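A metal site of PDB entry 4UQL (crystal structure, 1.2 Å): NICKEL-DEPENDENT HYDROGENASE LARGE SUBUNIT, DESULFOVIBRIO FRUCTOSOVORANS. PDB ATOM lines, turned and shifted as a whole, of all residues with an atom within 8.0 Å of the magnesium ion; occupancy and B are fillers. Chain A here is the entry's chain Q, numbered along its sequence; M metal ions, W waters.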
ATOM      1  N   PHE A  63     -14.688 -13.042  15.211  1.00  0.00           N
ATOM      2  CA  PHE A  63     -15.748 -12.085  15.571  1.00  0.00           C
ATOM      3  C   PHE A  63     -15.149 -10.962  16.402  1.00  0.00           C
ATOM      4  O   PHE A  63     -14.359 -11.244  17.303  1.00  0.00           O
ATOM      5  CB  PHE A  63     -16.822 -12.798  16.404  1.00  0.00           C
ATOM      6  CG  PHE A  63     -17.968 -11.924  16.847  1.00  0.00           C
ATOM      7  CD1 PHE A  63     -19.006 -11.651  15.984  1.00  0.00           C
ATOM      8  CD2 PHE A  63     -17.988 -11.351  18.120  1.00  0.00           C
ATOM      9  CE1 PHE A  63     -20.054 -10.845  16.380  1.00  0.00           C
ATOM     10  CE2 PHE A  63     -19.036 -10.527  18.530  1.00  0.00           C
ATOM     11  CZ  PHE A  63     -20.085 -10.286  17.650  1.00  0.00           C
ATOM     12  N   GLU A  67     -21.150  -3.895  16.309  1.00  0.00           N
ATOM     13  CA  GLU A  67     -22.545  -3.484  16.525  1.00  0.00           C
ATOM     14  C   GLU A  67     -22.863  -3.468  18.025  1.00  0.00           C
ATOM     15  O   GLU A  67     -23.578  -2.608  18.505  1.00  0.00           O
ATOM     16  CB  GLU A  67     -23.481  -4.449  15.791  1.00  0.00           C
ATOM     17  CG  GLU A  67     -23.314  -4.368  14.289  1.00  0.00           C
ATOM     18  CD  GLU A  67     -23.729  -5.626  13.559  1.00  0.00           C
ATOM     19  OE1 GLU A  67     -23.747  -6.707  14.189  1.00  0.00           O
ATOM     20  OE2 GLU A  67     -24.030  -5.532  12.331  1.00  0.00           O
ATOM     21  N   GLU A 348     -31.521 -10.590   7.548  1.00  0.00           N
ATOM     22  CA  GLU A 348     -30.405 -11.472   7.819  1.00  0.00           C
ATOM     23  C   GLU A 348     -30.865 -12.642   8.663  1.00  0.00           C
ATOM     24  O   GLU A 348     -31.606 -12.470   9.637  1.00  0.00           O
ATOM     25  CB  GLU A 348     -29.237 -10.761   8.536  1.00  0.00           C
ATOM     26  CG  GLU A 348     -28.586  -9.652   7.717  1.00  0.00           C
ATOM     27  CD  GLU A 348     -27.545  -8.939   8.507  1.00  0.00           C
ATOM     28  OE1 GLU A 348     -27.870  -8.174   9.458  1.00  0.00           O
ATOM     29  OE2 GLU A 348     -26.359  -9.098   8.137  1.00  0.00           O
ATOM     30  N   TYR A 355     -24.621 -17.496  16.301  1.00  0.00           N
ATOM     31  CA  TYR A 355     -25.464 -16.586  17.066  1.00  0.00           C
ATOM     32  C   TYR A 355     -26.564 -17.364  17.720  1.00  0.00           C
ATOM     33  O   TYR A 355     -26.834 -18.511  17.368  1.00  0.00           O
ATOM     34  CB  TYR A 355     -26.028 -15.484  16.150  1.00  0.00           C
ATOM     35  CG  TYR A 355     -24.915 -14.631  15.569  1.00  0.00           C
ATOM     36  CD1 TYR A 355     -24.298 -13.645  16.316  1.00  0.00           C
ATOM     37  CD2 TYR A 355     -24.455 -14.865  14.310  1.00  0.00           C
ATOM     38  CE1 TYR A 355     -23.242 -12.893  15.804  1.00  0.00           C
ATOM     39  CE2 TYR A 355     -23.399 -14.144  13.803  1.00  0.00           C
ATOM     40  CZ  TYR A 355     -22.771 -13.162  14.563  1.00  0.00           C
ATOM     41  OH  TYR A 355     -21.706 -12.456  14.030  1.00  0.00           O
ATOM     42  N   PRO A 364     -32.611  -5.263   9.136  1.00  0.00           N
ATOM     43  CA  PRO A 364     -31.529  -4.687   9.942  1.00  0.00           C
ATOM     44  C   PRO A 364     -31.923  -3.581  10.958  1.00  0.00           C
ATOM     45  O   PRO A 364     -31.242  -3.381  11.953  1.00  0.00           O
ATOM     46  CB  PRO A 364     -30.514  -4.202   8.904  1.00  0.00           C
ATOM     47  CG  PRO A 364     -30.830  -4.954   7.697  1.00  0.00           C
ATOM     48  CD  PRO A 364     -32.290  -5.201   7.695  1.00  0.00           C
ATOM     49  N   GLY A 367     -32.226  -5.638  13.793  1.00  0.00           N
ATOM     50  CA  GLY A 367     -31.165  -6.625  13.918  1.00  0.00           C
ATOM     51  C   GLY A 367     -30.765  -6.952  15.339  1.00  0.00           C
ATOM     52  O   GLY A 367     -30.911  -6.125  16.248  1.00  0.00           O
ATOM     53  N   VAL A 368     -30.232  -8.142  15.493  1.00  0.00           N
ATOM     54  CA  VAL A 368     -29.787  -8.653  16.763  1.00  0.00           C
ATOM     55  C   VAL A 368     -28.422  -9.324  16.554  1.00  0.00           C
ATOM     56  O   VAL A 368     -28.228 -10.073  15.576  1.00  0.00           O
ATOM     57  CB  VAL A 368     -30.752  -9.763  17.263  1.00  0.00           C
ATOM     58  CG1 VAL A 368     -30.312 -10.271  18.644  1.00  0.00           C
ATOM     59  CG2 VAL A 368     -32.196  -9.303  17.259  1.00  0.00           C
ATOM     60  N   THR A 369     -27.465  -9.038  17.444  1.00  0.00           N
ATOM     61  CA  THR A 369     -26.126  -9.615  17.344  1.00  0.00           C
ATOM     62  C   THR A 369     -25.766 -10.235  18.711  1.00  0.00           C
ATOM     63  O   THR A 369     -25.252  -9.544  19.590  1.00  0.00           O
ATOM     64  CB  THR A 369     -25.118  -8.529  16.901  1.00  0.00           C
ATOM     65  OG1 THR A 369     -25.631  -7.921  15.707  1.00  0.00           O
ATOM     66  CG2 THR A 369     -23.774  -9.108  16.654  1.00  0.00           C
ATOM     67  N   TRP A 384     -19.090 -16.953  11.675  1.00  0.00           N
ATOM     68  CA  TRP A 384     -19.407 -15.746  12.371  1.00  0.00           C
ATOM     69  C   TRP A 384     -20.138 -14.715  11.501  1.00  0.00           C
ATOM     70  O   TRP A 384     -20.583 -13.723  12.000  1.00  0.00           O
ATOM     71  CB  TRP A 384     -18.116 -15.108  12.929  1.00  0.00           C
ATOM     72  CG  TRP A 384     -17.562 -15.804  14.148  1.00  0.00           C
ATOM     73  CD1 TRP A 384     -16.414 -16.550  14.228  1.00  0.00           C
ATOM     74  CD2 TRP A 384     -18.179 -15.879  15.435  1.00  0.00           C
ATOM     75  NE1 TRP A 384     -16.269 -17.055  15.505  1.00  0.00           N
ATOM     76  CE2 TRP A 384     -17.330 -16.629  16.271  1.00  0.00           C
ATOM     77  CE3 TRP A 384     -19.360 -15.341  15.973  1.00  0.00           C
ATOM     78  CZ2 TRP A 384     -17.633 -16.855  17.618  1.00  0.00           C
ATOM     79  CZ3 TRP A 384     -19.644 -15.591  17.298  1.00  0.00           C
ATOM     80  CH2 TRP A 384     -18.787 -16.329  18.093  1.00  0.00           C
ATOM     81  N   MET A 385     -20.211 -14.919  10.199  1.00  0.00           N
ATOM     82  CA  MET A 385     -21.069 -14.060   9.395  1.00  0.00           C
ATOM     83  C   MET A 385     -22.532 -14.479   9.557  1.00  0.00           C
ATOM     84  O   MET A 385     -22.845 -15.683   9.603  1.00  0.00           O
ATOM     85  CB  MET A 385     -20.740 -14.107   7.923  1.00  0.00           C
ATOM     86  CG  MET A 385     -19.396 -13.480   7.583  1.00  0.00           C
ATOM     87  SD  MET A 385     -19.280 -13.195   5.811  1.00  0.00           S
ATOM     88  CE  MET A 385     -17.527 -12.986   5.628  1.00  0.00           C
ATOM     89  N   LYS A 386     -23.428 -13.478   9.554  1.00  0.00           N
ATOM     90  CA  LYS A 386     -24.869 -13.694   9.295  1.00  0.00           C
ATOM     91  C   LYS A 386     -25.039 -13.995   7.800  1.00  0.00           C
ATOM     92  O   LYS A 386     -24.092 -13.886   6.995  1.00  0.00           O
ATOM     93  CB  LYS A 386     -25.667 -12.465   9.723  1.00  0.00           C
ATOM     94  CG  LYS A 386     -25.479 -12.081  11.161  1.00  0.00           C
ATOM     95  CD  LYS A 386     -26.390 -10.908  11.533  1.00  0.00           C
ATOM     96  CE  LYS A 386     -26.232 -10.515  12.989  1.00  0.00           C
ATOM     97  NZ  LYS A 386     -26.817  -9.161  13.260  1.00  0.00           N
ATOM     98  N   PRO A 388     -27.257 -12.676   4.910  1.00  0.00           N
ATOM     99  CA  PRO A 388     -28.235 -11.737   4.363  1.00  0.00           C
ATOM    100  C   PRO A 388     -28.972 -12.343   3.172  1.00  0.00           C
ATOM    101  O   PRO A 388     -28.363 -12.989   2.339  1.00  0.00           O
ATOM    102  CB  PRO A 388     -27.377 -10.530   3.939  1.00  0.00           C
ATOM    103  CG  PRO A 388     -26.029 -10.757   4.560  1.00  0.00           C
ATOM    104  CD  PRO A 388     -25.891 -12.260   4.582  1.00  0.00           C
ATOM    105  N   SER A 494     -24.722  -1.421   3.562  1.00  0.00           N
ATOM    106  CA  SER A 494     -25.727  -0.647   4.272  1.00  0.00           C
ATOM    107  C   SER A 494     -25.466  -0.646   5.757  1.00  0.00           C
ATOM    108  O   SER A 494     -25.127  -1.673   6.343  1.00  0.00           O
ATOM    109  CB  SER A 494     -27.123  -1.124   3.869  1.00  0.00           C
ATOM    110  OG  SER A 494     -27.327  -2.503   4.110  1.00  0.00           O
ATOM    111  N   TRP A 496     -27.445   0.740   9.354  1.00  0.00           N
ATOM    112  CA  TRP A 496     -28.820   1.016   9.781  1.00  0.00           C
ATOM    113  C   TRP A 496     -28.821   1.383  11.258  1.00  0.00           C
ATOM    114  O   TRP A 496     -28.303   0.603  12.078  1.00  0.00           O
ATOM    115  CB  TRP A 496     -29.632  -0.248   9.618  1.00  0.00           C
ATOM    116  CG  TRP A 496     -29.565  -0.883   8.251  1.00  0.00           C
ATOM    117  CD1 TRP A 496     -28.541  -1.621   7.772  1.00  0.00           C
ATOM    118  CD2 TRP A 496     -30.578  -0.871   7.244  1.00  0.00           C
ATOM    119  NE1 TRP A 496     -28.851  -2.092   6.513  1.00  0.00           N
ATOM    120  CE2 TRP A 496     -30.098  -1.644   6.166  1.00  0.00           C
ATOM    121  CE3 TRP A 496     -31.855  -0.310   7.145  1.00  0.00           C
ATOM    122  CZ2 TRP A 496     -30.836  -1.855   5.009  1.00  0.00           C
ATOM    123  CZ3 TRP A 496     -32.584  -0.530   5.970  1.00  0.00           C
ATOM    124  CH2 TRP A 496     -32.073  -1.270   4.930  1.00  0.00           C
ATOM    125  N   PHE A 507     -27.394  -0.401  16.022  1.00  0.00           N
ATOM    126  CA  PHE A 507     -26.613  -0.030  14.851  1.00  0.00           C
ATOM    127  C   PHE A 507     -26.193  -1.328  14.213  1.00  0.00           C
ATOM    128  O   PHE A 507     -25.523  -2.168  14.832  1.00  0.00           O
ATOM    129  CB  PHE A 507     -25.371   0.789  15.220  1.00  0.00           C
ATOM    130  CG  PHE A 507     -24.841   1.567  14.075  1.00  0.00           C
ATOM    131  CD1 PHE A 507     -24.170   0.904  13.043  1.00  0.00           C
ATOM    132  CD2 PHE A 507     -25.032   2.944  13.975  1.00  0.00           C
ATOM    133  CE1 PHE A 507     -23.689   1.594  11.948  1.00  0.00           C
ATOM    134  CE2 PHE A 507     -24.531   3.630  12.870  1.00  0.00           C
ATOM    135  CZ  PHE A 507     -23.899   2.940  11.854  1.00  0.00           C
ATOM    136  N   GLN A 508     -26.634  -1.558  12.963  1.00  0.00           N
ATOM    137  CA  GLN A 508     -26.408  -2.802  12.246  1.00  0.00           C
ATOM    138  C   GLN A 508     -25.703  -2.522  10.934  1.00  0.00           C
ATOM    139  O   GLN A 508     -26.160  -1.679  10.144  1.00  0.00           O
ATOM    140  CB  GLN A 508     -27.725  -3.531  12.024  1.00  0.00           C
ATOM    141  CG  GLN A 508     -28.401  -4.000  13.302  1.00  0.00           C
ATOM    142  CD  GLN A 508     -27.718  -5.188  13.952  1.00  0.00           C
ATOM    143  OE1 GLN A 508     -27.201  -6.088  13.285  1.00  0.00           O
ATOM    144  NE2 GLN A 508     -27.693  -5.225  15.274  1.00  0.00           N
ATOM    145  N   LEU A 509     -24.629  -3.286  10.695  1.00  0.00           N
ATOM    146  CA  LEU A 509     -23.941  -3.256   9.407  1.00  0.00           C
ATOM    147  C   LEU A 509     -24.347  -4.519   8.645  1.00  0.00           C
ATOM    148  O   LEU A 509     -24.340  -5.612   9.189  1.00  0.00           O
ATOM    149  CB  LEU A 509     -22.422  -3.297   9.588  1.00  0.00           C
ATOM    150  CG  LEU A 509     -21.739  -2.125  10.275  1.00  0.00           C
ATOM    151  CD1 LEU A 509     -21.989  -2.074  11.730  1.00  0.00           C
ATOM    152  CD2 LEU A 509     -20.236  -2.191  10.059  1.00  0.00           C
ATOM    153  N   VAL A 510     -24.661  -4.351   7.365  1.00  0.00           N
ATOM    154  CA  VAL A 510     -24.845  -5.463   6.431  1.00  0.00           C
ATOM    155  C   VAL A 510     -23.904  -5.181   5.257  1.00  0.00           C
ATOM    156  O   VAL A 510     -24.068  -4.175   4.561  1.00  0.00           O
ATOM    157  CB  VAL A 510     -26.306  -5.545   5.939  1.00  0.00           C
ATOM    158  CG1 VAL A 510     -26.504  -6.795   5.128  1.00  0.00           C
ATOM    159  CG2 VAL A 510     -27.259  -5.573   7.099  1.00  0.00           C
ATOM    160  N   VAL A 511     -22.886  -6.018   5.096  1.00  0.00           N
ATOM    161  CA  VAL A 511     -21.717  -5.645   4.365  1.00  0.00           C
ATOM    162  C   VAL A 511     -21.605  -6.539   3.106  1.00  0.00           C
ATOM    163  O   VAL A 511     -22.081  -7.666   3.094  1.00  0.00           O
ATOM    164  CB  VAL A 511     -20.518  -5.749   5.279  1.00  0.00           C
ATOM    165  CG1 VAL A 511     -19.234  -5.223   4.676  1.00  0.00           C
ATOM    166  CG2 VAL A 511     -20.790  -4.914   6.543  1.00  0.00           C
ATOM    167  N   THR A 514     -20.597 -10.022   3.613  1.00  0.00           N
ATOM    168  CA  THR A 514     -21.676 -10.745   4.304  1.00  0.00           C
ATOM    169  C   THR A 514     -22.588 -11.373   3.247  1.00  0.00           C
ATOM    170  O   THR A 514     -22.909 -12.581   3.330  1.00  0.00           O
ATOM    171  CB  THR A 514     -22.469  -9.882   5.311  1.00  0.00           C
ATOM    172  OG1 THR A 514     -21.617  -8.904   5.927  1.00  0.00           O
ATOM    173  CG2 THR A 514     -23.114 -10.760   6.321  1.00  0.00           C
ATOM    174  N   CYS A 560     -14.793  -7.107   7.300  1.00  0.00           N
ATOM    175  CA  CYS A 560     -16.028  -6.486   6.789  1.00  0.00           C
ATOM    176  C   CYS A 560     -17.235  -7.362   7.021  1.00  0.00           C
ATOM    177  O   CYS A 560     -18.278  -6.897   7.502  1.00  0.00           O
ATOM    178  CB  CYS A 560     -15.961  -6.235   5.289  1.00  0.00           C
ATOM    179  SG  CYS A 560     -15.398  -4.604   4.803  1.00  0.00           S
ATOM    180  N   GLY A 561     -17.105  -8.629   6.640  1.00  0.00           N
ATOM    181  CA  GLY A 561     -18.304  -9.434   6.604  1.00  0.00           C
ATOM    182  C   GLY A 561     -18.886  -9.742   7.984  1.00  0.00           C
ATOM    183  O   GLY A 561     -20.111  -9.839   8.119  1.00  0.00           O
ATOM    184  N   VAL A 562     -18.003  -9.918   8.971  1.00  0.00           N
ATOM    185  CA  VAL A 562     -18.445 -10.220  10.354  1.00  0.00           C
ATOM    186  C   VAL A 562     -18.585  -8.983  11.221  1.00  0.00           C
ATOM    187  O   VAL A 562     -19.513  -8.895  12.031  1.00  0.00           O
ATOM    188  CB  VAL A 562     -17.453 -11.164  11.018  1.00  0.00           C
ATOM    189  CG1 VAL A 562     -17.892 -11.415  12.452  1.00  0.00           C
ATOM    190  CG2 VAL A 562     -17.336 -12.485  10.290  1.00  0.00           C
ATOM    191  N   HIS A 563     -17.644  -8.033  11.095  1.00  0.00           N
ATOM    192  CA  HIS A 563     -17.613  -6.858  11.966  1.00  0.00           C
ATOM    193  C   HIS A 563     -17.851  -7.245  13.434  1.00  0.00           C
ATOM    194  O   HIS A 563     -18.545  -6.514  14.155  1.00  0.00           O
ATOM    195  CB  HIS A 563     -18.511  -5.720  11.443  1.00  0.00           C
ATOM    196  CG  HIS A 563     -19.841  -6.160  10.938  1.00  0.00           C
ATOM    197  ND1 HIS A 563     -20.021  -6.689   9.671  1.00  0.00           N
ATOM    198  CD2 HIS A 563     -21.057  -6.198  11.531  1.00  0.00           C
ATOM    199  CE1 HIS A 563     -21.297  -7.039   9.514  1.00  0.00           C
ATOM    200  NE2 HIS A 563     -21.943  -6.749  10.635  1.00  0.00           N
ATOM    201  OXT HIS A 563     -17.196  -8.202  13.924  1.00  0.00           O
HETATM  202 MG    MG M   1     -24.108  -6.981  10.779  1.00  0.00          MG
HETATM  203  O   HOH W   1     -23.919  -8.483  12.272  1.00  0.00           O
HETATM  204  O   HOH W   2     -24.120  -8.469   9.337  1.00  0.00           O
HETATM  205  O   HOH W   3     -26.179  -7.047  11.010  1.00  0.00           O
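The side-chain carboxylate (OE2) of Glu 67 sits close to the side-chain amide oxygen (OE1) of Gln 508.
The side-chain carboxylate (OE1) of Glu 67 lies within hydrogen-bond range of the side-chain hydroxyl (OG1) of Thr 369 (2.7 Å).
ND1 of His 563 is in hydrogen-bond range of O of Cys 560.
Within 4 Å of the magnesium ion: Glu 67, Leu 509 and His 563.
The nearest printed residue that does not touch the magnesium ion is Glu 348 (4.1 Å).
The magnesium ion is bound by water W2, at 2.1 Å.
The magnesium ion is bound by water W3, 2.1 Å away.
O of Leu 509 binds the magnesium ion, 2.1 Å away.
The magnesium ion is bound by OE2 of Glu 67 (2.1 Å).
Water W1 binds the magnesium ion, at 2.1 Å.
NE2 of His 563 is bound to the magnesium ion, at 2.2 Å.
The magnesium ion has six donor atoms within binding distance.
Water W3 lies within hydrogen-bond range of OE1 of Glu 348 (2.6 Å), OE1 of Gln 508 (2.7 Å) and NZ of Lys 386 (3.2 Å).
Water W1 bridges the side-chain carboxylate of Glu 67 (2.6 Å) and the side-chain amino group of Lys 386 (3.1 Å).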
